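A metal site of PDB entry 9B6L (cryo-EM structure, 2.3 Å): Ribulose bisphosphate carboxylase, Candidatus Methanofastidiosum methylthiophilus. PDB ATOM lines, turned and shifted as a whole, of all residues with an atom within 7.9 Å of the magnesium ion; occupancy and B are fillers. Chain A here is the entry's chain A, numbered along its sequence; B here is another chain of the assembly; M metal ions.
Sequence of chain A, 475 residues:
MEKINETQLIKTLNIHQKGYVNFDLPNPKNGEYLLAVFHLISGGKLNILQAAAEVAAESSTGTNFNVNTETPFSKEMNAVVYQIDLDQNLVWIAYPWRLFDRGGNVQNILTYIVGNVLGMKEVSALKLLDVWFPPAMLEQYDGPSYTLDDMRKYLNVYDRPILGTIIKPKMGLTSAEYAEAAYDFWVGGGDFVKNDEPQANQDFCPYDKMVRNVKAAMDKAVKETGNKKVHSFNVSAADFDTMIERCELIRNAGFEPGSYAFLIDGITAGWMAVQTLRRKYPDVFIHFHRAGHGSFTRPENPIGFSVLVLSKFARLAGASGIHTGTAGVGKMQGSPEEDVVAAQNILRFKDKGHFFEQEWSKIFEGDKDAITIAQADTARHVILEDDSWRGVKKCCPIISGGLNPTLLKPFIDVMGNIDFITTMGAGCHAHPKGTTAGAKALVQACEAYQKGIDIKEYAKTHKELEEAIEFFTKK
The side-chain carboxylate (OD2) of Asp 196 lies within salt-bridge range of the side-chain amino group (NZ) of Lys 170 (2.7 Å). The backbone NH (N) of Asp 196 lies within hydrogen-bond range of the side-chain amide oxygen (OE1) of Gln 199 (3.2 Å). OE2 of Glu 197 sits at hydrogen-bond distance from ND2 of Asn 116 of chain B, 3.3 Å away. NE2 of His 289 lies close to OE1 of Glu 197, 3.2 Å away. OQ1 of KCX 194 sits at hydrogen-bond distance from a ring nitrogen (NE2) of His 289, at 3.1 Å.
Merely in contact with the magnesium ion: Asn 116 of chain B. The nearest printed residue that does not touch the magnesium ion is Lys 170 (4.1 Å).
OD1 of Asp 196 is bound to the magnesium ion. The magnesium ion is bound by OE1 of Glu 197, 2.3 Å away. The magnesium ion is bound by OQ2 of KCX 194 (2.4 Å). The magnesium ion has three donor atoms within binding distance.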
ATOM      1  N   ILE A 166     -14.810   4.327 -14.570  1.00  0.00           N
ATOM      2  CA  ILE A 166     -14.088   4.977 -15.650  1.00  0.00           C
ATOM      3  C   ILE A 166     -12.708   5.320 -15.124  1.00  0.00           C
ATOM      4  O   ILE A 166     -12.523   5.616 -13.931  1.00  0.00           O
ATOM      5  CB  ILE A 166     -14.805   6.251 -16.163  1.00  0.00           C
ATOM      6  CG1 ILE A 166     -15.011   7.246 -15.010  1.00  0.00           C
ATOM      7  CG2 ILE A 166     -16.136   5.890 -16.815  1.00  0.00           C
ATOM      8  CD1 ILE A 166     -15.369   8.636 -15.466  1.00  0.00           C
ATOM      9  N   ILE A 167     -11.716   5.255 -16.002  1.00  0.00           N
ATOM     10  CA  ILE A 167     -10.344   5.568 -15.633  1.00  0.00           C
ATOM     11  C   ILE A 167     -10.139   7.063 -15.741  1.00  0.00           C
ATOM     12  O   ILE A 167     -10.502   7.689 -16.742  1.00  0.00           O
ATOM     13  CB  ILE A 167      -9.350   4.794 -16.525  1.00  0.00           C
ATOM     14  CG1 ILE A 167      -9.428   3.296 -16.228  1.00  0.00           C
ATOM     15  CG2 ILE A 167      -7.932   5.317 -16.332  1.00  0.00           C
ATOM     16  CD1 ILE A 167      -9.422   2.962 -14.752  1.00  0.00           C
ATOM     17  N   LYS A 168      -9.564   7.653 -14.699  1.00  0.00           N
ATOM     18  CA  LYS A 168      -9.237   9.068 -14.652  1.00  0.00           C
ATOM     19  C   LYS A 168      -7.721   9.239 -14.595  1.00  0.00           C
ATOM     20  O   LYS A 168      -7.081   8.623 -13.730  1.00  0.00           O
ATOM     21  CB  LYS A 168      -9.883   9.752 -13.442  1.00  0.00           C
ATOM     22  CG  LYS A 168     -11.401   9.818 -13.510  1.00  0.00           C
ATOM     23  CD  LYS A 168     -11.860  10.810 -14.565  1.00  0.00           C
ATOM     24  CE  LYS A 168     -13.154  11.484 -14.149  1.00  0.00           C
ATOM     25  NZ  LYS A 168     -13.719  12.322 -15.241  1.00  0.00           N
ATOM     26  N   LYS A 170      -9.429  10.660 -18.262  1.00  0.00           N
ATOM     27  CA  LYS A 170     -10.134  10.007 -19.357  1.00  0.00           C
ATOM     28  C   LYS A 170      -9.177   9.635 -20.477  1.00  0.00           C
ATOM     29  O   LYS A 170      -9.199   8.505 -20.984  1.00  0.00           O
ATOM     30  CB  LYS A 170     -11.221  10.937 -19.899  1.00  0.00           C
ATOM     31  CG  LYS A 170     -12.583  10.784 -19.278  1.00  0.00           C
ATOM     32  CD  LYS A 170     -13.378  12.098 -19.339  1.00  0.00           C
ATOM     33  CE  LYS A 170     -13.014  12.958 -20.550  1.00  0.00           C
ATOM     34  NZ  LYS A 170     -13.376  12.354 -21.862  1.00  0.00           N
ATOM     35  N   MET A 171      -8.324  10.572 -20.871  1.00  0.00           N
ATOM     36  CA  MET A 171      -7.393  10.398 -21.979  1.00  0.00           C
ATOM     37  C   MET A 171      -6.033  10.919 -21.557  1.00  0.00           C
ATOM     38  O   MET A 171      -5.862  11.502 -20.485  1.00  0.00           O
ATOM     39  CB  MET A 171      -7.884  11.126 -23.238  1.00  0.00           C
ATOM     40  CG  MET A 171      -9.195  10.598 -23.802  1.00  0.00           C
ATOM     41  SD  MET A 171      -9.090   8.981 -24.594  1.00  0.00           S
ATOM     42  CE  MET A 171      -7.422   9.002 -25.237  1.00  0.00           C
ATOM     43  N   KCX A 194     -14.447   0.395 -18.108  1.00  0.00           N
ATOM     44  CA  KCX A 194     -14.784   0.783 -19.471  1.00  0.00           C
ATOM     45  CB  KCX A 194     -16.184   1.402 -19.521  1.00  0.00           C
ATOM     46  CG  KCX A 194     -16.350   2.633 -18.658  1.00  0.00           C
ATOM     47  CD  KCX A 194     -17.753   3.206 -18.771  1.00  0.00           C
ATOM     48  CE  KCX A 194     -18.050   3.668 -20.192  1.00  0.00           C
ATOM     49  NZ  KCX A 194     -17.087   4.711 -20.648  1.00  0.00           N
ATOM     50  C   KCX A 194     -13.767   1.737 -20.059  1.00  0.00           C
ATOM     51  O   KCX A 194     -13.220   2.602 -19.366  1.00  0.00           O
ATOM     52  CX  KCX A 194     -17.276   5.981 -20.320  1.00  0.00           C
ATOM     53  OQ1 KCX A 194     -18.255   6.314 -19.643  1.00  0.00           O
ATOM     54  OQ2 KCX A 194     -16.477   6.835 -20.696  1.00  0.00           O
ATOM     55  N   ASN A 195     -13.506   1.581 -21.352  1.00  0.00           N
ATOM     56  CA  ASN A 195     -12.783   2.599 -22.109  1.00  0.00           C
ATOM     57  C   ASN A 195     -13.586   3.886 -22.082  1.00  0.00           C
ATOM     58  O   ASN A 195     -14.813   3.854 -22.036  1.00  0.00           O
ATOM     59  CB  ASN A 195     -12.570   2.153 -23.564  1.00  0.00           C
ATOM     60  CG  ASN A 195     -11.313   1.326 -23.747  1.00  0.00           C
ATOM     61  OD1 ASN A 195     -10.401   1.383 -22.927  1.00  0.00           O
ATOM     62  ND2 ASN A 195     -11.259   0.559 -24.815  1.00  0.00           N
ATOM     63  N   ASP A 196     -12.889   5.018 -22.087  1.00  0.00           N
ATOM     64  CA  ASP A 196     -13.573   6.279 -22.316  1.00  0.00           C
ATOM     65  C   ASP A 196     -14.233   6.251 -23.690  1.00  0.00           C
ATOM     66  O   ASP A 196     -13.726   5.647 -24.636  1.00  0.00           O
ATOM     67  CB  ASP A 196     -12.598   7.452 -22.229  1.00  0.00           C
ATOM     68  CG  ASP A 196     -13.281   8.770 -21.946  1.00  0.00           C
ATOM     69  OD1 ASP A 196     -14.318   8.770 -21.259  1.00  0.00           O
ATOM     70  OD2 ASP A 196     -12.784   9.818 -22.403  1.00  0.00           O
ATOM     71  N   GLU A 197     -15.399   6.896 -23.788  1.00  0.00           N
ATOM     72  CA  GLU A 197     -16.162   6.814 -25.035  1.00  0.00           C
ATOM     73  C   GLU A 197     -15.410   7.329 -26.264  1.00  0.00           C
ATOM     74  O   GLU A 197     -15.697   6.825 -27.362  1.00  0.00           O
ATOM     75  CB  GLU A 197     -17.525   7.501 -24.858  1.00  0.00           C
ATOM     76  CG  GLU A 197     -17.547   9.006 -24.827  1.00  0.00           C
ATOM     77  CD  GLU A 197     -17.158   9.577 -23.489  1.00  0.00           C
ATOM     78  OE1 GLU A 197     -17.121   8.802 -22.505  1.00  0.00           O
ATOM     79  OE2 GLU A 197     -16.876  10.782 -23.405  1.00  0.00           O
ATOM     80  N   PRO A 198     -14.460   8.265 -26.191  1.00  0.00           N
ATOM     81  CA  PRO A 198     -13.594   8.519 -27.349  1.00  0.00           C
ATOM     82  C   PRO A 198     -12.247   7.804 -27.311  1.00  0.00           C
ATOM     83  O   PRO A 198     -11.417   8.065 -28.187  1.00  0.00           O
ATOM     84  CB  PRO A 198     -13.382  10.041 -27.266  1.00  0.00           C
ATOM     85  CG  PRO A 198     -13.940  10.492 -25.948  1.00  0.00           C
ATOM     86  CD  PRO A 198     -14.213   9.271 -25.145  1.00  0.00           C
ATOM     87  N   GLN A 199     -12.010   6.920 -26.339  1.00  0.00           N
ATOM     88  CA  GLN A 199     -10.741   6.201 -26.247  1.00  0.00           C
ATOM     89  C   GLN A 199     -10.648   5.195 -27.375  1.00  0.00           C
ATOM     90  O   GLN A 199     -11.476   4.281 -27.478  1.00  0.00           O
ATOM     91  CB  GLN A 199     -10.616   5.515 -24.894  1.00  0.00           C
ATOM     92  CG  GLN A 199      -9.467   4.529 -24.801  1.00  0.00           C
ATOM     93  CD  GLN A 199      -8.995   4.314 -23.379  1.00  0.00           C
ATOM     94  OE1 GLN A 199      -9.714   4.622 -22.417  1.00  0.00           O
ATOM     95  NE2 GLN A 199      -7.788   3.793 -23.230  1.00  0.00           N
ATOM     96  N   LEU A 263     -17.909  -1.489 -26.487  1.00  0.00           N
ATOM     97  CA  LEU A 263     -18.521  -0.171 -26.319  1.00  0.00           C
ATOM     98  C   LEU A 263     -18.646   0.497 -27.671  1.00  0.00           C
ATOM     99  O   LEU A 263     -17.694   0.499 -28.465  1.00  0.00           O
ATOM    100  CB  LEU A 263     -17.706   0.691 -25.363  1.00  0.00           C
ATOM    101  CG  LEU A 263     -18.355   1.998 -24.912  1.00  0.00           C
ATOM    102  CD1 LEU A 263     -17.972   2.305 -23.474  1.00  0.00           C
ATOM    103  CD2 LEU A 263     -17.985   3.173 -25.809  1.00  0.00           C
ATOM    104  N   HIS A 289     -22.910   3.535 -25.555  1.00  0.00           N
ATOM    105  CA  HIS A 289     -22.611   4.836 -24.996  1.00  0.00           C
ATOM    106  C   HIS A 289     -23.365   5.898 -25.786  1.00  0.00           C
ATOM    107  O   HIS A 289     -23.294   5.929 -27.021  1.00  0.00           O
ATOM    108  CB  HIS A 289     -21.111   5.117 -25.025  1.00  0.00           C
ATOM    109  CG  HIS A 289     -20.660   6.085 -23.972  1.00  0.00           C
ATOM    110  ND1 HIS A 289     -20.894   7.439 -24.073  1.00  0.00           N
ATOM    111  CD2 HIS A 289     -20.016   5.894 -22.797  1.00  0.00           C
ATOM    112  CE1 HIS A 289     -20.403   8.047 -22.999  1.00  0.00           C
ATOM    113  NE2 HIS A 289     -19.869   7.133 -22.221  1.00  0.00           N
ATOM    114  N   ALA A 291     -23.018   9.232 -25.870  1.00  0.00           N
ATOM    115  CA  ALA A 291     -22.376  10.531 -25.998  1.00  0.00           C
ATOM    116  C   ALA A 291     -22.909  11.270 -27.217  1.00  0.00           C
ATOM    117  O   ALA A 291     -22.951  10.732 -28.316  1.00  0.00           O
ATOM    118  CB  ALA A 291     -20.854  10.371 -26.090  1.00  0.00           C
ATOM    119  N   HIS A 323     -26.302   3.772 -21.129  1.00  0.00           N
ATOM    120  CA  HIS A 323     -26.123   4.683 -20.014  1.00  0.00           C
ATOM    121  C   HIS A 323     -27.431   5.371 -19.648  1.00  0.00           C
ATOM    122  O   HIS A 323     -28.262   5.683 -20.501  1.00  0.00           O
ATOM    123  CB  HIS A 323     -25.061   5.726 -20.339  1.00  0.00           C
ATOM    124  CG  HIS A 323     -23.655   5.214 -20.247  1.00  0.00           C
ATOM    125  ND1 HIS A 323     -22.817   5.520 -19.202  1.00  0.00           N
ATOM    126  CD2 HIS A 323     -22.946   4.413 -21.071  1.00  0.00           C
ATOM    127  CE1 HIS A 323     -21.655   4.929 -19.375  1.00  0.00           C
ATOM    128  NE2 HIS A 323     -21.703   4.249 -20.512  1.00  0.00           N
ATOM    129  N   SER A 400     -23.601   6.330 -14.341  1.00  0.00           N
ATOM    130  CA  SER A 400     -22.330   7.026 -14.457  1.00  0.00           C
ATOM    131  C   SER A 400     -22.326   8.246 -13.560  1.00  0.00           C
ATOM    132  O   SER A 400     -23.295   9.023 -13.550  1.00  0.00           O
ATOM    133  CB  SER A 400     -22.056   7.437 -15.903  1.00  0.00           C
ATOM    134  OG  SER A 400     -20.667   7.435 -16.197  1.00  0.00           O
ATOM    135  N   GLU B  58     -14.231  17.747 -19.753  1.00  0.00           N
ATOM    136  CA  GLU B  58     -15.074  16.629 -20.163  1.00  0.00           C
ATOM    137  C   GLU B  58     -14.914  16.277 -21.634  1.00  0.00           C
ATOM    138  O   GLU B  58     -15.213  15.147 -22.022  1.00  0.00           O
ATOM    139  CB  GLU B  58     -16.540  16.938 -19.841  1.00  0.00           C
ATOM    140  CG  GLU B  58     -17.532  15.839 -20.175  1.00  0.00           C
ATOM    141  CD  GLU B  58     -17.123  14.486 -19.603  1.00  0.00           C
ATOM    142  OE1 GLU B  58     -16.892  14.405 -18.376  1.00  0.00           O
ATOM    143  OE2 GLU B  58     -17.024  13.509 -20.376  1.00  0.00           O
ATOM    144  N   GLY B  62     -10.942  15.043 -18.865  1.00  0.00           N
ATOM    145  CA  GLY B  62     -11.773  14.800 -17.687  1.00  0.00           C
ATOM    146  C   GLY B  62     -11.024  14.736 -16.375  1.00  0.00           C
ATOM    147  O   GLY B  62     -11.282  13.839 -15.566  1.00  0.00           O
ATOM    148  N   THR B 111     -17.646  12.823 -30.790  1.00  0.00           N
ATOM    149  CA  THR B 111     -17.734  12.274 -29.444  1.00  0.00           C
ATOM    150  C   THR B 111     -16.984  13.137 -28.444  1.00  0.00           C
ATOM    151  O   THR B 111     -17.465  13.382 -27.337  1.00  0.00           O
ATOM    152  CB  THR B 111     -17.178  10.846 -29.435  1.00  0.00           C
ATOM    153  OG1 THR B 111     -18.014  10.003 -30.240  1.00  0.00           O
ATOM    154  CG2 THR B 111     -17.104  10.299 -28.035  1.00  0.00           C
ATOM    155  N   ASN B 116     -20.354  14.092 -24.591  1.00  0.00           N
ATOM    156  CA  ASN B 116     -20.859  14.168 -23.226  1.00  0.00           C
ATOM    157  C   ASN B 116     -21.029  15.596 -22.722  1.00  0.00           C
ATOM    158  O   ASN B 116     -21.745  15.807 -21.748  1.00  0.00           O
ATOM    159  CB  ASN B 116     -19.922  13.417 -22.280  1.00  0.00           C
ATOM    160  CG  ASN B 116     -20.211  11.927 -22.230  1.00  0.00           C
ATOM    161  OD1 ASN B 116     -21.066  11.427 -22.960  1.00  0.00           O
ATOM    162  ND2 ASN B 116     -19.491  11.214 -21.373  1.00  0.00           N
HETATM  163 MG    MG M   1     -16.178   9.170 -20.478  1.00  0.00          MG
